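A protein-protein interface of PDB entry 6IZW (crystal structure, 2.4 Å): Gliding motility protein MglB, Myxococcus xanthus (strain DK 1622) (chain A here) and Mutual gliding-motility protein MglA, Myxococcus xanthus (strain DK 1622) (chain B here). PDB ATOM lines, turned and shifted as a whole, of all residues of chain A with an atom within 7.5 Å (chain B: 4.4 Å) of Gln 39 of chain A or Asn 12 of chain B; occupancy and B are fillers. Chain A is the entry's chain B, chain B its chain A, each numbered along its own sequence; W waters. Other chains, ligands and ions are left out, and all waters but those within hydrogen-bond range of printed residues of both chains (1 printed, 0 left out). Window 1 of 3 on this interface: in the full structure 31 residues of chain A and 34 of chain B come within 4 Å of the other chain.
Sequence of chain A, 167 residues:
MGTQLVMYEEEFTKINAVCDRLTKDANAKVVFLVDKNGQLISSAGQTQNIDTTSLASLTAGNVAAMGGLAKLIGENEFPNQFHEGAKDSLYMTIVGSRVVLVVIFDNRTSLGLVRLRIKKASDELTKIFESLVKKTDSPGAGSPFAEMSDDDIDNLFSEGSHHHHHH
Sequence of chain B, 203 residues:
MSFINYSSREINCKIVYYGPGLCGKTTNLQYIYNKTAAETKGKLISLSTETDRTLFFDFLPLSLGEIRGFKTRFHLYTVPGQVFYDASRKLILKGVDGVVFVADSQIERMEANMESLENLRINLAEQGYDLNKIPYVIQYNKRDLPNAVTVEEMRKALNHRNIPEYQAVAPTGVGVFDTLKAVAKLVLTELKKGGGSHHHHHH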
ATOM      1  N   LEU A   5      -9.938   1.796 -31.183  1.00  0.00           N
ATOM      2  CA  LEU A   5     -10.731   1.059 -30.218  1.00  0.00           C
ATOM      3  C   LEU A   5     -10.363   1.502 -28.806  1.00  0.00           C
ATOM      4  O   LEU A   5      -9.184   1.696 -28.486  1.00  0.00           O
ATOM      5  CB  LEU A   5     -10.531  -0.455 -30.388  1.00  0.00           C
ATOM      6  CG  LEU A   5     -11.498  -1.088 -31.396  1.00  0.00           C
ATOM      7  CD1 LEU A   5     -11.546  -2.611 -31.266  1.00  0.00           C
ATOM      8  CD2 LEU A   5     -12.900  -0.486 -31.265  1.00  0.00           C
ATOM      9  N   LEU A  33      -6.489 -13.237 -22.515  1.00  0.00           N
ATOM     10  CA  LEU A  33      -7.368 -12.878 -23.612  1.00  0.00           C
ATOM     11  C   LEU A  33      -6.601 -11.962 -24.558  1.00  0.00           C
ATOM     12  O   LEU A  33      -5.981 -10.994 -24.110  1.00  0.00           O
ATOM     13  CB  LEU A  33      -8.626 -12.188 -23.081  1.00  0.00           C
ATOM     14  CG  LEU A  33      -9.790 -12.087 -24.060  1.00  0.00           C
ATOM     15  CD1 LEU A  33     -10.387 -13.471 -24.266  1.00  0.00           C
ATOM     16  CD2 LEU A  33     -10.861 -11.071 -23.613  1.00  0.00           C
ATOM     17  N   VAL A  34      -6.631 -12.267 -25.859  1.00  0.00           N
ATOM     18  CA  VAL A  34      -5.819 -11.562 -26.847  1.00  0.00           C
ATOM     19  C   VAL A  34      -6.666 -11.253 -28.073  1.00  0.00           C
ATOM     20  O   VAL A  34      -7.423 -12.103 -28.554  1.00  0.00           O
ATOM     21  CB  VAL A  34      -4.561 -12.366 -27.246  1.00  0.00           C
ATOM     22  CG1 VAL A  34      -4.923 -13.757 -27.718  1.00  0.00           C
ATOM     23  CG2 VAL A  34      -3.782 -11.641 -28.334  1.00  0.00           C
ATOM     24  N   ASP A  35      -6.551 -10.027 -28.563  1.00  0.00           N
ATOM     25  CA  ASP A  35      -7.126  -9.662 -29.846  1.00  0.00           C
ATOM     26  C   ASP A  35      -6.410 -10.399 -30.979  1.00  0.00           C
ATOM     27  O   ASP A  35      -5.242 -10.785 -30.866  1.00  0.00           O
ATOM     28  CB  ASP A  35      -7.014  -8.146 -30.042  1.00  0.00           C
ATOM     29  CG  ASP A  35      -7.865  -7.637 -31.180  1.00  0.00           C
ATOM     30  OD1 ASP A  35      -7.587  -7.976 -32.356  1.00  0.00           O
ATOM     31  OD2 ASP A  35      -8.818  -6.880 -30.894  1.00  0.00           O
ATOM     32  N   LYS A  36      -7.117 -10.571 -32.094  1.00  0.00           N
ATOM     33  CA  LYS A  36      -6.516 -11.231 -33.241  1.00  0.00           C
ATOM     34  C   LYS A  36      -5.295 -10.472 -33.755  1.00  0.00           C
ATOM     35  O   LYS A  36      -4.331 -11.090 -34.229  1.00  0.00           O
ATOM     36  CB  LYS A  36      -7.559 -11.399 -34.347  1.00  0.00           C
ATOM     37  CG  LYS A  36      -8.300 -12.737 -34.279  1.00  0.00           C
ATOM     38  CD  LYS A  36      -9.237 -12.915 -35.462  1.00  0.00           C
ATOM     39  CE  LYS A  36     -10.192 -14.086 -35.213  1.00  0.00           C
ATOM     40  NZ  LYS A  36     -11.008 -14.393 -36.412  1.00  0.00           N
ATOM     41  N   ASN A  37      -5.299  -9.144 -33.651  1.00  0.00           N
ATOM     42  CA  ASN A  37      -4.193  -8.366 -34.181  1.00  0.00           C
ATOM     43  C   ASN A  37      -2.962  -8.430 -33.293  1.00  0.00           C
ATOM     44  O   ASN A  37      -1.949  -7.825 -33.644  1.00  0.00           O
ATOM     45  CB  ASN A  37      -4.616  -6.906 -34.408  1.00  0.00           C
ATOM     46  CG  ASN A  37      -5.016  -6.177 -33.114  1.00  0.00           C
ATOM     47  OD1 ASN A  37      -4.509  -6.455 -32.017  1.00  0.00           O
ATOM     48  ND2 ASN A  37      -5.927  -5.224 -33.252  1.00  0.00           N
ATOM     49  N   GLY A  38      -3.035  -9.131 -32.160  1.00  0.00           N
ATOM     50  CA  GLY A  38      -1.913  -9.307 -31.259  1.00  0.00           C
ATOM     51  C   GLY A  38      -2.056  -8.602 -29.926  1.00  0.00           C
ATOM     52  O   GLY A  38      -1.249  -8.859 -29.023  1.00  0.00           O
ATOM     53  N   GLN A  39      -3.036  -7.713 -29.773  1.00  0.00           N
ATOM     54  CA  GLN A  39      -3.138  -6.883 -28.575  1.00  0.00           C
ATOM     55  C   GLN A  39      -3.671  -7.682 -27.378  1.00  0.00           C
ATOM     56  O   GLN A  39      -4.793  -8.201 -27.411  1.00  0.00           O
ATOM     57  CB  GLN A  39      -4.044  -5.684 -28.853  1.00  0.00           C
ATOM     58  CG  GLN A  39      -4.386  -4.874 -27.602  1.00  0.00           C
ATOM     59  CD  GLN A  39      -3.155  -4.247 -26.977  1.00  0.00           C
ATOM     60  OE1 GLN A  39      -2.343  -3.646 -27.672  1.00  0.00           O
ATOM     61  NE2 GLN A  39      -2.987  -4.421 -25.668  1.00  0.00           N
ATOM     62  N   LEU A  40      -2.872  -7.758 -26.315  1.00  0.00           N
ATOM     63  CA  LEU A  40      -3.281  -8.408 -25.076  1.00  0.00           C
ATOM     64  C   LEU A  40      -4.354  -7.578 -24.375  1.00  0.00           C
ATOM     65  O   LEU A  40      -4.150  -6.390 -24.104  1.00  0.00           O
ATOM     66  CB  LEU A  40      -2.073  -8.590 -24.160  1.00  0.00           C
ATOM     67  CG  LEU A  40      -2.351  -9.085 -22.738  1.00  0.00           C
ATOM     68  CD1 LEU A  40      -3.014 -10.449 -22.784  1.00  0.00           C
ATOM     69  CD2 LEU A  40      -1.068  -9.157 -21.913  1.00  0.00           C
ATOM     70  N   ILE A  41      -5.497  -8.193 -24.082  1.00  0.00           N
ATOM     71  CA  ILE A  41      -6.607  -7.493 -23.447  1.00  0.00           C
ATOM     72  C   ILE A  41      -6.683  -7.789 -21.954  1.00  0.00           C
ATOM     73  O   ILE A  41      -6.883  -6.876 -21.152  1.00  0.00           O
ATOM     74  CB  ILE A  41      -7.938  -7.823 -24.153  1.00  0.00           C
ATOM     75  CG1 ILE A  41      -7.851  -7.446 -25.625  1.00  0.00           C
ATOM     76  CG2 ILE A  41      -9.073  -7.064 -23.507  1.00  0.00           C
ATOM     77  CD1 ILE A  41      -8.880  -8.138 -26.498  1.00  0.00           C
ATOM     78  N   SER A  42      -6.512  -9.047 -21.546  1.00  0.00           N
ATOM     79  CA  SER A  42      -6.511  -9.376 -20.121  1.00  0.00           C
ATOM     80  C   SER A  42      -5.780 -10.690 -19.888  1.00  0.00           C
ATOM     81  O   SER A  42      -5.733 -11.556 -20.764  1.00  0.00           O
ATOM     82  CB  SER A  42      -7.931  -9.482 -19.562  1.00  0.00           C
ATOM     83  OG  SER A  42      -8.788  -8.536 -20.177  1.00  0.00           O
ATOM     84  N   THR A  53       3.032 -10.634 -22.680  1.00  0.00           N
ATOM     85  CA  THR A  53       3.018  -9.830 -23.899  1.00  0.00           C
ATOM     86  C   THR A  53       3.543 -10.635 -25.086  1.00  0.00           C
ATOM     87  O   THR A  53       2.948 -10.610 -26.170  1.00  0.00           O
ATOM     88  CB  THR A  53       3.825  -8.546 -23.705  1.00  0.00           C
ATOM     89  OG1 THR A  53       3.070  -7.640 -22.892  1.00  0.00           O
ATOM     90  CG2 THR A  53       4.088  -7.878 -25.036  1.00  0.00           C
ATOM     91  N   ALA A  56       0.815 -13.349 -25.934  1.00  0.00           N
ATOM     92  CA  ALA A  56      -0.272 -12.809 -26.743  1.00  0.00           C
ATOM     93  C   ALA A  56       0.130 -12.656 -28.204  1.00  0.00           C
ATOM     94  O   ALA A  56      -0.707 -12.817 -29.102  1.00  0.00           O
ATOM     95  CB  ALA A  56      -0.716 -11.459 -26.183  1.00  0.00           C
ATOM     96  N   SER A  57       1.397 -12.322 -28.462  1.00  0.00           N
ATOM     97  CA  SER A  57       1.822 -12.033 -29.828  1.00  0.00           C
ATOM     98  C   SER A  57       1.995 -13.319 -30.632  1.00  0.00           C
ATOM     99  O   SER A  57       1.605 -13.386 -31.800  1.00  0.00           O
ATOM    100  CB  SER A  57       3.127 -11.226 -29.801  1.00  0.00           C
ATOM    101  OG  SER A  57       3.517 -10.842 -31.101  1.00  0.00           O
ATOM    102  N   ALA A  60      -1.628 -14.793 -31.287  1.00  0.00           N
ATOM    103  CA  ALA A  60      -2.367 -14.211 -32.397  1.00  0.00           C
ATOM    104  C   ALA A  60      -1.707 -14.535 -33.724  1.00  0.00           C
ATOM    105  O   ALA A  60      -2.391 -14.626 -34.751  1.00  0.00           O
ATOM    106  CB  ALA A  60      -2.503 -12.702 -32.217  1.00  0.00           C
ATOM    107  N   ARG A  98     -13.110 -11.098 -33.024  1.00  0.00           N
ATOM    108  CA  ARG A  98     -11.751 -10.570 -32.978  1.00  0.00           C
ATOM    109  C   ARG A  98     -10.992 -10.943 -31.713  1.00  0.00           C
ATOM    110  O   ARG A  98      -9.903 -10.407 -31.491  1.00  0.00           O
ATOM    111  CB  ARG A  98     -11.750  -9.027 -33.174  1.00  0.00           C
ATOM    112  CG  ARG A  98     -12.461  -8.202 -32.061  1.00  0.00           C
ATOM    113  CD  ARG A  98     -12.450  -6.637 -32.322  1.00  0.00           C
ATOM    114  NE  ARG A  98     -11.177  -5.922 -32.077  1.00  0.00           N
ATOM    115  CZ  ARG A  98     -10.394  -5.358 -33.017  1.00  0.00           C
ATOM    116  NH1 ARG A  98     -10.717  -5.390 -34.317  1.00  0.00           N
ATOM    117  NH2 ARG A  98      -9.262  -4.743 -32.625  1.00  0.00           N
ATOM    118  N   VAL A  99     -11.479 -11.892 -30.921  1.00  0.00           N
ATOM    119  CA  VAL A  99     -10.881 -12.186 -29.630  1.00  0.00           C
ATOM    120  C   VAL A  99     -10.508 -13.660 -29.585  1.00  0.00           C
ATOM    121  O   VAL A  99     -11.024 -14.479 -30.345  1.00  0.00           O
ATOM    122  CB  VAL A  99     -11.837 -11.814 -28.482  1.00  0.00           C
ATOM    123  CG1 VAL A  99     -11.106 -11.735 -27.182  1.00  0.00           C
ATOM    124  CG2 VAL A  99     -12.491 -10.486 -28.784  1.00  0.00           C
ATOM    125  N   VAL A 100      -9.574 -13.985 -28.693  1.00  0.00           N
ATOM    126  CA  VAL A 100      -9.077 -15.342 -28.512  1.00  0.00           C
ATOM    127  C   VAL A 100      -8.847 -15.540 -27.023  1.00  0.00           C
ATOM    128  O   VAL A 100      -8.110 -14.765 -26.405  1.00  0.00           O
ATOM    129  CB  VAL A 100      -7.764 -15.600 -29.278  1.00  0.00           C
ATOM    130  CG1 VAL A 100      -7.199 -16.976 -28.943  1.00  0.00           C
ATOM    131  CG2 VAL A 100      -7.958 -15.438 -30.772  1.00  0.00           C
ATOM    132  N   SER B   2      -5.325   0.910 -33.178  1.00  0.00           N
ATOM    133  CA  SER B   2      -4.863   1.187 -31.823  1.00  0.00           C
ATOM    134  C   SER B   2      -5.910   0.783 -30.794  1.00  0.00           C
ATOM    135  O   SER B   2      -7.079   0.588 -31.116  1.00  0.00           O
ATOM    136  CB  SER B   2      -4.536   2.670 -31.671  1.00  0.00           C
ATOM    137  OG  SER B   2      -5.683   3.444 -31.966  1.00  0.00           O
ATOM    138  N   PHE B   3      -5.480   0.683 -29.544  1.00  0.00           N
ATOM    139  CA  PHE B   3      -6.328   0.224 -28.458  1.00  0.00           C
ATOM    140  C   PHE B   3      -5.997   1.032 -27.206  1.00  0.00           C
ATOM    141  O   PHE B   3      -4.858   0.986 -26.725  1.00  0.00           O
ATOM    142  CB  PHE B   3      -6.116  -1.273 -28.221  1.00  0.00           C
ATOM    143  CG  PHE B   3      -6.841  -1.810 -27.017  1.00  0.00           C
ATOM    144  CD1 PHE B   3      -8.223  -1.914 -27.011  1.00  0.00           C
ATOM    145  CD2 PHE B   3      -6.140  -2.213 -25.893  1.00  0.00           C
ATOM    146  CE1 PHE B   3      -8.886  -2.412 -25.902  1.00  0.00           C
ATOM    147  CE2 PHE B   3      -6.798  -2.709 -24.785  1.00  0.00           C
ATOM    148  CZ  PHE B   3      -8.172  -2.811 -24.790  1.00  0.00           C
ATOM    149  N   GLU B  10      -3.421   3.201 -20.808  1.00  0.00           N
ATOM    150  CA  GLU B  10      -2.414   2.706 -21.736  1.00  0.00           C
ATOM    151  C   GLU B  10      -2.873   2.937 -23.161  1.00  0.00           C
ATOM    152  O   GLU B  10      -3.986   2.554 -23.529  1.00  0.00           O
ATOM    153  CB  GLU B  10      -2.127   1.225 -21.509  1.00  0.00           C
ATOM    154  CG  GLU B  10      -1.194   0.969 -20.341  1.00  0.00           C
ATOM    155  CD  GLU B  10      -1.184  -0.489 -19.899  1.00  0.00           C
ATOM    156  OE1 GLU B  10      -1.829  -1.339 -20.570  1.00  0.00           O
ATOM    157  OE2 GLU B  10      -0.531  -0.776 -18.867  1.00  0.00           O
ATOM    158  N   ILE B  11      -2.020   3.583 -23.952  1.00  0.00           N
ATOM    159  CA  ILE B  11      -2.224   3.714 -25.392  1.00  0.00           C
ATOM    160  C   ILE B  11      -1.329   2.697 -26.087  1.00  0.00           C
ATOM    161  O   ILE B  11      -0.110   2.671 -25.860  1.00  0.00           O
ATOM    162  CB  ILE B  11      -1.927   5.145 -25.872  1.00  0.00           C
ATOM    163  CG1 ILE B  11      -2.740   6.157 -25.060  1.00  0.00           C
ATOM    164  CG2 ILE B  11      -2.203   5.288 -27.382  1.00  0.00           C
ATOM    165  CD1 ILE B  11      -2.150   7.532 -25.082  1.00  0.00           C
ATOM    166  N   ASN B  12      -1.937   1.860 -26.928  1.00  0.00           N
ATOM    167  CA  ASN B  12      -1.278   0.755 -27.632  1.00  0.00           C
ATOM    168  C   ASN B  12      -1.345   1.000 -29.128  1.00  0.00           C
ATOM    169  O   ASN B  12      -2.432   1.222 -29.676  1.00  0.00           O
ATOM    170  CB  ASN B  12      -1.947  -0.594 -27.341  1.00  0.00           C
ATOM    171  CG  ASN B  12      -2.068  -0.881 -25.877  1.00  0.00           C
ATOM    172  OD1 ASN B  12      -1.214  -1.543 -25.299  1.00  0.00           O
ATOM    173  ND2 ASN B  12      -3.138  -0.375 -25.257  1.00  0.00           N
ATOM    174  N   CYS B  13      -0.192   0.957 -29.786  1.00  0.00           N
ATOM    175  CA  CYS B  13      -0.112   1.203 -31.218  1.00  0.00           C
ATOM    176  C   CYS B  13       0.762   0.149 -31.870  1.00  0.00           C
ATOM    177  O   CYS B  13       1.771  -0.289 -31.304  1.00  0.00           O
ATOM    178  CB  CYS B  13       0.454   2.597 -31.517  1.00  0.00           C
ATOM    179  SG  CYS B  13      -0.609   3.946 -30.904  1.00  0.00           S
ATOM    180  N   ARG B  73       2.438   2.292 -25.360  1.00  0.00           N
ATOM    181  CA  ARG B  73       3.050   1.006 -25.683  1.00  0.00           C
ATOM    182  C   ARG B  73       3.023   0.844 -27.198  1.00  0.00           C
ATOM    183  O   ARG B  73       1.951   0.816 -27.805  1.00  0.00           O
ATOM    184  CB  ARG B  73       2.325  -0.145 -24.975  1.00  0.00           C
ATOM    185  CG  ARG B  73       2.389  -0.028 -23.452  1.00  0.00           C
ATOM    186  CD  ARG B  73       3.206  -1.142 -22.800  1.00  0.00           C
ATOM    187  NE  ARG B  73       3.612  -0.863 -21.415  1.00  0.00           N
ATOM    188  CZ  ARG B  73       2.784  -0.530 -20.425  1.00  0.00           C
ATOM    189  NH1 ARG B  73       1.480  -0.417 -20.652  1.00  0.00           N
ATOM    190  NH2 ARG B  73       3.258  -0.303 -19.201  1.00  0.00           N
ATOM    191  N   HIS B  75       3.922  -1.572 -30.301  1.00  0.00           N
ATOM    192  CA  HIS B  75       4.127  -2.974 -30.624  1.00  0.00           C
ATOM    193  C   HIS B  75       4.784  -2.976 -31.992  1.00  0.00           C
ATOM    194  O   HIS B  75       4.140  -2.627 -32.986  1.00  0.00           O
ATOM    195  CB  HIS B  75       2.793  -3.729 -30.606  1.00  0.00           C
ATOM    196  CG  HIS B  75       2.085  -3.650 -29.286  1.00  0.00           C
ATOM    197  ND1 HIS B  75       2.402  -4.472 -28.222  1.00  0.00           N
ATOM    198  CD2 HIS B  75       1.125  -2.802 -28.835  1.00  0.00           C
ATOM    199  CE1 HIS B  75       1.652  -4.151 -27.181  1.00  0.00           C
ATOM    200  NE2 HIS B  75       0.865  -3.143 -27.528  1.00  0.00           N
ATOM    201  N   ASP B  97      -1.278   0.415 -37.187  1.00  0.00           N
ATOM    202  CA  ASP B  97      -1.452   1.855 -37.022  1.00  0.00           C
ATOM    203  C   ASP B  97      -0.449   2.667 -37.819  1.00  0.00           C
ATOM    204  O   ASP B  97      -0.784   3.756 -38.276  1.00  0.00           O
ATOM    205  CB  ASP B  97      -1.366   2.222 -35.540  1.00  0.00           C
ATOM    206  CG  ASP B  97      -2.390   1.479 -34.723  1.00  0.00           C
ATOM    207  OD1 ASP B  97      -3.598   1.663 -35.023  1.00  0.00           O
ATOM    208  OD2 ASP B  97      -1.992   0.693 -33.830  1.00  0.00           O
HETATM  209  O   HOH W   1       1.261  -7.243 -29.940  1.00  0.00           O
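Gln 39 of chain A touches just these residues of chain B: Phe 3, Asn 12 and His 75. Of the printed residues of chain A, Asn 12 of chain B touches Gln 39 (3.1 Å). Of the printed residues of chain A, His 75 of chain B touches Gln 39 (3.3 Å). Of the printed residues of chain A, Ser 2 of chain B touches Leu 5 (3.1 Å). The nearest printed residue of chain A that does not touch His 75 of chain B is Thr 53 of chain A (4.9 Å).
Water W1 lies within hydrogen-bond range of O of Gly 38 of chain A and ND1 of His 75 of chain B.
Of the 18 printed residues of chain A, 2 touch a printed residue of chain B. Hydrophobic or aromatic side chains of chain A within 4 Å of the printed part of chain B: Leu 5. Among the printed residues, 5 pairs touch across the chains.
O of Leu 5 of chain A touches CA of Phe 3 of chain B, 3.2 Å away. Phe 3 of chain B touches Gln 39 of chain A (CD2 to CG, 3.6 Å).
The backbone carbonyl oxygen (O) of Cys 13 of chain B is in hydrogen-bond range of the backbone NH (N) of His 75 of chain B, at 2.7 Å. A ring nitrogen (NE2) of His 75 of chain B sits at hydrogen-bond distance from the side-chain amide oxygen (OD1) of Asn 12 of chain B (3.4 Å). The side-chain amide oxygen of Asn 37 of chain A is in hydrogen-bond range of the backbone NH of Gln 39 of chain A. The backbone carbonyl oxygen (O) of Phe 3 of chain B sits at hydrogen-bond distance from the side-chain amide nitrogen (ND2) of Asn 12 of chain B. The side-chain carboxylate of Asp 97 of chain B is in hydrogen-bond range of the backbone NH of Ser 2 of chain B, 2.6 Å away.
The side-chain amide oxygen of Gln 39 of chain A sits at hydrogen-bond distance from a ring nitrogen (NE2) of His 75 of chain B, at 3.3 Å. The backbone carbonyl oxygen of Ser 2 of chain B lies within hydrogen-bond range of the backbone NH of Leu 5 of chain A, 3.1 Å away. OD1 of Asn 12 of chain B sits close to OE1 of Gln 39 of chain A.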
